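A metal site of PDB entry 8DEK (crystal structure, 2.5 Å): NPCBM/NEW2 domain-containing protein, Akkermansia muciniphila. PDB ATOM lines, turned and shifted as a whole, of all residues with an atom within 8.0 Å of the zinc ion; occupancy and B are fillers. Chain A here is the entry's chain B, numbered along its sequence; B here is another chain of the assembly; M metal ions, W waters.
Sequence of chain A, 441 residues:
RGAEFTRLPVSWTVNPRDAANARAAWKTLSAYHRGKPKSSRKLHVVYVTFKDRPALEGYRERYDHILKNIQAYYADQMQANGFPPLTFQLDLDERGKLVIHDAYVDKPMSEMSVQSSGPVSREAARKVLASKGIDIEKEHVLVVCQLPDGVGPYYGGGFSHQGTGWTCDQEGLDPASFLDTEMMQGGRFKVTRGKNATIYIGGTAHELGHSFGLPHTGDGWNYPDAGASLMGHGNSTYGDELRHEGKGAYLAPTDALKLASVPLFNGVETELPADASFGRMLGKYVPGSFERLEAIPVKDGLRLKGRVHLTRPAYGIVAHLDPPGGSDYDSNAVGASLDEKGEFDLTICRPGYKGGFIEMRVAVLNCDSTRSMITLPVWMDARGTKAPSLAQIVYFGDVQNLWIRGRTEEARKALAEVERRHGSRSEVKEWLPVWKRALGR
NE2 of His 216 lies close to OH of Tyr 329 (3.3 Å). A ring nitrogen (ND1) of His 216 sits at hydrogen-bond distance from the side-chain carboxylate (OD1) of Asp 328, at 2.7 Å. ND1 of His 206 sits at hydrogen-bond distance from O of Leu 230 (2.9 Å). A ring nitrogen (ND1) of His 210 lies within hydrogen-bond range of the backbone carbonyl oxygen (O) of Leu 214.
Merely in contact with the zinc ion: Tyr 329 (3.6 Å). Four residues have an atom within 4 Å of the zinc ion: His 206, His 210, His 216 and Tyr 329. The nearest printed residue that does not touch the zinc ion is Lys 190 of chain B (4.5 Å).
A ring nitrogen (NE2) of His 216 binds the zinc ion (2.3 Å). A ring nitrogen (NE2) of His 206 binds the zinc ion, at 2.3 Å. NE2 of His 210 binds the zinc ion (2.3 Å). The zinc ion has three donor atoms within binding distance. Slightly farther from the zinc ion lies water W1 (2.6 Å). Slightly farther from the zinc ion lies water W2 (2.7 Å).
Water W2 bridges OE1 of Glu 207 (2.6 Å) and NZ of Lys 190 of chain B (3.0 Å).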
ATOM      1  N   TYR A 154     -33.397  -6.295  35.402  1.00  0.00           N
ATOM      2  CA  TYR A 154     -33.115  -7.476  34.593  1.00  0.00           C
ATOM      3  C   TYR A 154     -31.628  -7.424  34.292  1.00  0.00           C
ATOM      4  O   TYR A 154     -31.203  -6.820  33.306  1.00  0.00           O
ATOM      5  CB  TYR A 154     -33.962  -7.509  33.326  1.00  0.00           C
ATOM      6  CG  TYR A 154     -35.454  -7.532  33.568  1.00  0.00           C
ATOM      7  CD1 TYR A 154     -36.171  -6.352  33.753  1.00  0.00           C
ATOM      8  CD2 TYR A 154     -36.150  -8.742  33.620  1.00  0.00           C
ATOM      9  CE1 TYR A 154     -37.534  -6.373  33.975  1.00  0.00           C
ATOM     10  CE2 TYR A 154     -37.513  -8.764  33.842  1.00  0.00           C
ATOM     11  CZ  TYR A 154     -38.198  -7.584  34.025  1.00  0.00           C
ATOM     12  OH  TYR A 154     -39.551  -7.606  34.251  1.00  0.00           O
ATOM     13  N   TYR A 155     -30.835  -8.056  35.154  1.00  0.00           N
ATOM     14  CA  TYR A 155     -29.393  -7.866  35.132  1.00  0.00           C
ATOM     15  C   TYR A 155     -28.697  -9.150  35.564  1.00  0.00           C
ATOM     16  O   TYR A 155     -29.312 -10.050  36.135  1.00  0.00           O
ATOM     17  CB  TYR A 155     -28.978  -6.698  36.046  1.00  0.00           C
ATOM     18  CG  TYR A 155     -27.620  -6.118  35.767  1.00  0.00           C
ATOM     19  CD1 TYR A 155     -27.299  -5.606  34.508  1.00  0.00           C
ATOM     20  CD2 TYR A 155     -26.643  -6.058  36.759  1.00  0.00           C
ATOM     21  CE1 TYR A 155     -26.052  -5.072  34.248  1.00  0.00           C
ATOM     22  CE2 TYR A 155     -25.397  -5.524  36.499  1.00  0.00           C
ATOM     23  CZ  TYR A 155     -25.106  -5.029  35.254  1.00  0.00           C
ATOM     24  OH  TYR A 155     -23.862  -4.489  35.003  1.00  0.00           O
ATOM     25  N   GLY A 156     -27.397  -9.208  35.288  1.00  0.00           N
ATOM     26  CA  GLY A 156     -26.586 -10.344  35.670  1.00  0.00           C
ATOM     27  C   GLY A 156     -25.108 -10.018  35.681  1.00  0.00           C
ATOM     28  O   GLY A 156     -24.598  -9.354  34.771  1.00  0.00           O
ATOM     29  N   GLY A 203     -34.520 -14.571  29.250  1.00  0.00           N
ATOM     30  CA  GLY A 203     -33.715 -13.527  29.851  1.00  0.00           C
ATOM     31  C   GLY A 203     -33.030 -13.999  31.120  1.00  0.00           C
ATOM     32  O   GLY A 203     -31.840 -13.749  31.325  1.00  0.00           O
ATOM     33  N   HIS A 206     -30.186 -15.920  30.360  1.00  0.00           N
ATOM     34  CA  HIS A 206     -29.138 -15.049  29.867  1.00  0.00           C
ATOM     35  C   HIS A 206     -28.417 -14.343  31.009  1.00  0.00           C
ATOM     36  O   HIS A 206     -27.191 -14.233  31.008  1.00  0.00           O
ATOM     37  CB  HIS A 206     -29.735 -14.037  28.887  1.00  0.00           C
ATOM     38  CG  HIS A 206     -28.735 -13.062  28.332  1.00  0.00           C
ATOM     39  ND1 HIS A 206     -28.107 -13.246  27.123  1.00  0.00           N
ATOM     40  CD2 HIS A 206     -28.282 -11.881  28.822  1.00  0.00           C
ATOM     41  CE1 HIS A 206     -27.302 -12.226  26.887  1.00  0.00           C
ATOM     42  NE2 HIS A 206     -27.386 -11.384  27.905  1.00  0.00           N
ATOM     43  N   GLU A 207     -29.168 -13.850  32.004  1.00  0.00           N
ATOM     44  CA  GLU A 207     -28.536 -13.177  33.139  1.00  0.00           C
ATOM     45  C   GLU A 207     -27.749 -14.162  33.989  1.00  0.00           C
ATOM     46  O   GLU A 207     -26.689 -13.821  34.528  1.00  0.00           O
ATOM     47  CB  GLU A 207     -29.593 -12.461  33.992  1.00  0.00           C
ATOM     48  CG  GLU A 207     -30.625 -11.667  33.202  1.00  0.00           C
ATOM     49  CD  GLU A 207     -30.096 -10.338  32.675  1.00  0.00           C
ATOM     50  OE1 GLU A 207     -28.879 -10.090  32.764  1.00  0.00           O
ATOM     51  OE2 GLU A 207     -30.917  -9.549  32.161  1.00  0.00           O
ATOM     52  N   HIS A 210     -24.460 -14.590  32.535  1.00  0.00           N
ATOM     53  CA  HIS A 210     -23.626 -13.462  32.938  1.00  0.00           C
ATOM     54  C   HIS A 210     -23.078 -13.660  34.351  1.00  0.00           C
ATOM     55  O   HIS A 210     -21.906 -13.358  34.614  1.00  0.00           O
ATOM     56  CB  HIS A 210     -24.438 -12.166  32.861  1.00  0.00           C
ATOM     57  CG  HIS A 210     -24.551 -11.601  31.482  1.00  0.00           C
ATOM     58  ND1 HIS A 210     -23.458 -11.400  30.657  1.00  0.00           N
ATOM     59  CD2 HIS A 210     -25.620 -11.181  30.773  1.00  0.00           C
ATOM     60  CE1 HIS A 210     -23.851 -10.878  29.515  1.00  0.00           C
ATOM     61  NE2 HIS A 210     -25.172 -10.740  29.554  1.00  0.00           N
ATOM     62  N   LEU A 214     -19.874 -15.162  31.956  1.00  0.00           N
ATOM     63  CA  LEU A 214     -19.933 -15.213  30.500  1.00  0.00           C
ATOM     64  C   LEU A 214     -20.240 -13.837  29.948  1.00  0.00           C
ATOM     65  O   LEU A 214     -21.288 -13.263  30.297  1.00  0.00           O
ATOM     66  CB  LEU A 214     -20.987 -16.211  30.035  1.00  0.00           C
ATOM     67  CG  LEU A 214     -20.708 -17.704  30.231  1.00  0.00           C
ATOM     68  CD1 LEU A 214     -21.859 -18.523  29.661  1.00  0.00           C
ATOM     69  CD2 LEU A 214     -19.390 -18.089  29.580  1.00  0.00           C
ATOM     70  N   PRO A 215     -19.379 -13.271  29.110  1.00  0.00           N
ATOM     71  CA  PRO A 215     -19.757 -12.045  28.397  1.00  0.00           C
ATOM     72  C   PRO A 215     -20.680 -12.355  27.230  1.00  0.00           C
ATOM     73  O   PRO A 215     -21.123 -13.504  27.061  1.00  0.00           O
ATOM     74  CB  PRO A 215     -18.412 -11.480  27.911  1.00  0.00           C
ATOM     75  CG  PRO A 215     -17.347 -12.314  28.587  1.00  0.00           C
ATOM     76  CD  PRO A 215     -17.978 -13.638  28.864  1.00  0.00           C
ATOM     77  N   HIS A 216     -20.988 -11.353  26.417  1.00  0.00           N
ATOM     78  CA  HIS A 216     -21.846 -11.550  25.258  1.00  0.00           C
ATOM     79  C   HIS A 216     -21.084 -12.229  24.130  1.00  0.00           C
ATOM     80  O   HIS A 216     -19.898 -11.964  23.909  1.00  0.00           O
ATOM     81  CB  HIS A 216     -22.416 -10.221  24.774  1.00  0.00           C
ATOM     82  CG  HIS A 216     -23.590  -9.745  25.575  1.00  0.00           C
ATOM     83  ND1 HIS A 216     -23.867  -8.404  25.773  1.00  0.00           N
ATOM     84  CD2 HIS A 216     -24.561 -10.424  26.227  1.00  0.00           C
ATOM     85  CE1 HIS A 216     -24.959  -8.285  26.505  1.00  0.00           C
ATOM     86  NE2 HIS A 216     -25.397  -9.501  26.798  1.00  0.00           N
ATOM     87  N   LEU A 230     -27.355 -18.101  23.025  1.00  0.00           N
ATOM     88  CA  LEU A 230     -28.039 -17.681  24.254  1.00  0.00           C
ATOM     89  C   LEU A 230     -27.412 -16.407  24.827  1.00  0.00           C
ATOM     90  O   LEU A 230     -28.126 -15.510  25.282  1.00  0.00           O
ATOM     91  CB  LEU A 230     -28.012 -18.808  25.284  1.00  0.00           C
ATOM     92  CG  LEU A 230     -28.447 -18.401  26.694  1.00  0.00           C
ATOM     93  CD1 LEU A 230     -29.958 -18.432  26.823  1.00  0.00           C
ATOM     94  CD2 LEU A 230     -27.788 -19.286  27.747  1.00  0.00           C
ATOM     95  N   MET A 231     -26.087 -16.327  24.816  1.00  0.00           N
ATOM     96  CA  MET A 231     -25.407 -15.138  25.315  1.00  0.00           C
ATOM     97  C   MET A 231     -25.356 -14.019  24.279  1.00  0.00           C
ATOM     98  O   MET A 231     -24.710 -12.995  24.526  1.00  0.00           O
ATOM     99  CB  MET A 231     -24.003 -15.496  25.793  1.00  0.00           C
ATOM    100  CG  MET A 231     -23.996 -16.309  27.091  1.00  0.00           C
ATOM    101  SD  MET A 231     -25.116 -15.768  28.406  1.00  0.00           S
ATOM    102  CE  MET A 231     -24.753 -14.017  28.527  1.00  0.00           C
ATOM    103  N   GLY A 232     -25.999 -14.216  23.129  1.00  0.00           N
ATOM    104  CA  GLY A 232     -26.169 -13.145  22.165  1.00  0.00           C
ATOM    105  C   GLY A 232     -27.601 -12.672  22.151  1.00  0.00           C
ATOM    106  O   GLY A 232     -28.080 -12.112  23.141  1.00  0.00           O
ATOM    107  N   ASN A 235     -31.492 -14.769  24.183  1.00  0.00           N
ATOM    108  CA  ASN A 235     -32.362 -14.476  25.324  1.00  0.00           C
ATOM    109  C   ASN A 235     -33.793 -14.220  24.882  1.00  0.00           C
ATOM    110  O   ASN A 235     -34.738 -14.455  25.654  1.00  0.00           O
ATOM    111  CB  ASN A 235     -31.824 -13.267  26.088  1.00  0.00           C
ATOM    112  CG  ASN A 235     -31.937 -11.980  25.310  1.00  0.00           C
ATOM    113  OD1 ASN A 235     -31.141 -11.717  24.405  1.00  0.00           O
ATOM    114  ND2 ASN A 235     -32.927 -11.158  25.647  1.00  0.00           N
ATOM    115  N   LEU A 282     -16.712  -9.511  31.613  1.00  0.00           N
ATOM    116  CA  LEU A 282     -17.043 -10.383  32.738  1.00  0.00           C
ATOM    117  C   LEU A 282     -16.057 -11.541  32.829  1.00  0.00           C
ATOM    118  O   LEU A 282     -15.588 -12.073  31.818  1.00  0.00           O
ATOM    119  CB  LEU A 282     -18.468 -10.912  32.594  1.00  0.00           C
ATOM    120  CG  LEU A 282     -19.561  -9.932  33.015  1.00  0.00           C
ATOM    121  CD1 LEU A 282     -20.904 -10.354  32.449  1.00  0.00           C
ATOM    122  CD2 LEU A 282     -19.629  -9.814  34.532  1.00  0.00           C
ATOM    123  N   ASP A 328     -20.852  -5.825  22.175  1.00  0.00           N
ATOM    124  CA  ASP A 328     -20.455  -7.215  22.352  1.00  0.00           C
ATOM    125  C   ASP A 328     -21.470  -8.183  21.754  1.00  0.00           C
ATOM    126  O   ASP A 328     -21.130  -9.353  21.536  1.00  0.00           O
ATOM    127  CB  ASP A 328     -20.255  -7.510  23.840  1.00  0.00           C
ATOM    128  CG  ASP A 328     -21.309  -6.866  24.717  1.00  0.00           C
ATOM    129  OD1 ASP A 328     -22.453  -6.697  24.241  1.00  0.00           O
ATOM    130  OD2 ASP A 328     -20.999  -6.524  25.869  1.00  0.00           O
ATOM    131  N   TYR A 329     -22.684  -7.719  21.456  1.00  0.00           N
ATOM    132  CA  TYR A 329     -23.695  -8.571  20.830  1.00  0.00           C
ATOM    133  C   TYR A 329     -23.303  -8.977  19.417  1.00  0.00           C
ATOM    134  O   TYR A 329     -23.806  -9.993  18.911  1.00  0.00           O
ATOM    135  CB  TYR A 329     -25.043  -7.854  20.792  1.00  0.00           C
ATOM    136  CG  TYR A 329     -25.868  -7.974  22.041  1.00  0.00           C
ATOM    137  CD1 TYR A 329     -26.191  -9.220  22.569  1.00  0.00           C
ATOM    138  CD2 TYR A 329     -26.336  -6.842  22.707  1.00  0.00           C
ATOM    139  CE1 TYR A 329     -26.952  -9.332  23.722  1.00  0.00           C
ATOM    140  CE2 TYR A 329     -27.097  -6.955  23.860  1.00  0.00           C
ATOM    141  CZ  TYR A 329     -27.397  -8.201  24.359  1.00  0.00           C
ATOM    142  OH  TYR A 329     -28.156  -8.319  25.503  1.00  0.00           O
ATOM    143  N   MET B 183     -26.574   0.510  23.703  1.00  0.00           N
ATOM    144  CA  MET B 183     -27.494  -0.421  24.344  1.00  0.00           C
ATOM    145  C   MET B 183     -28.152   0.229  25.551  1.00  0.00           C
ATOM    146  O   MET B 183     -27.534   1.019  26.263  1.00  0.00           O
ATOM    147  CB  MET B 183     -26.744  -1.700  24.753  1.00  0.00           C
ATOM    148  CG  MET B 183     -26.416  -2.612  23.575  1.00  0.00           C
ATOM    149  SD  MET B 183     -27.826  -3.496  22.850  1.00  0.00           S
ATOM    150  CE  MET B 183     -28.897  -3.708  24.268  1.00  0.00           C
ATOM    151  N   GLN B 185     -29.518  -1.414  28.386  1.00  0.00           N
ATOM    152  CA  GLN B 185     -29.005  -2.017  29.611  1.00  0.00           C
ATOM    153  C   GLN B 185     -30.029  -2.051  30.735  1.00  0.00           C
ATOM    154  O   GLN B 185     -30.805  -1.107  30.911  1.00  0.00           O
ATOM    155  N   GLY B 186     -30.035  -3.140  31.489  1.00  0.00           N
ATOM    156  CA  GLY B 186     -30.840  -3.270  32.689  1.00  0.00           C
ATOM    157  C   GLY B 186     -32.317  -3.470  32.455  1.00  0.00           C
ATOM    158  O   GLY B 186     -33.098  -3.447  33.408  1.00  0.00           O
ATOM    159  N   GLY B 187     -32.731  -3.676  31.199  1.00  0.00           N
ATOM    160  CA  GLY B 187     -34.133  -3.888  30.885  1.00  0.00           C
ATOM    161  C   GLY B 187     -34.410  -5.318  30.473  1.00  0.00           C
ATOM    162  O   GLY B 187     -33.489  -6.042  30.096  1.00  0.00           O
ATOM    163  N   LYS B 190     -33.502  -6.624  25.601  1.00  0.00           N
ATOM    164  CA  LYS B 190     -32.113  -6.296  25.279  1.00  0.00           C
ATOM    165  C   LYS B 190     -32.070  -5.693  23.876  1.00  0.00           C
ATOM    166  O   LYS B 190     -31.877  -6.382  22.878  1.00  0.00           O
ATOM    167  CB  LYS B 190     -31.237  -7.532  25.374  1.00  0.00           C
ATOM    168  CG  LYS B 190     -31.373  -8.281  26.694  1.00  0.00           C
ATOM    169  CD  LYS B 190     -31.197  -7.346  27.875  1.00  0.00           C
ATOM    170  CE  LYS B 190     -31.056  -8.120  29.179  1.00  0.00           C
ATOM    171  NZ  LYS B 190     -30.442  -7.298  30.245  1.00  0.00           N
HETATM  172 ZN    ZN M   1     -26.735  -9.310  28.656  1.00  0.00          ZN
HETATM  173  O   HOH W   1     -26.012  -7.338  30.192  1.00  0.00           O
HETATM  174  O   HOH W   2     -27.781  -8.510  31.038  1.00  0.00           O
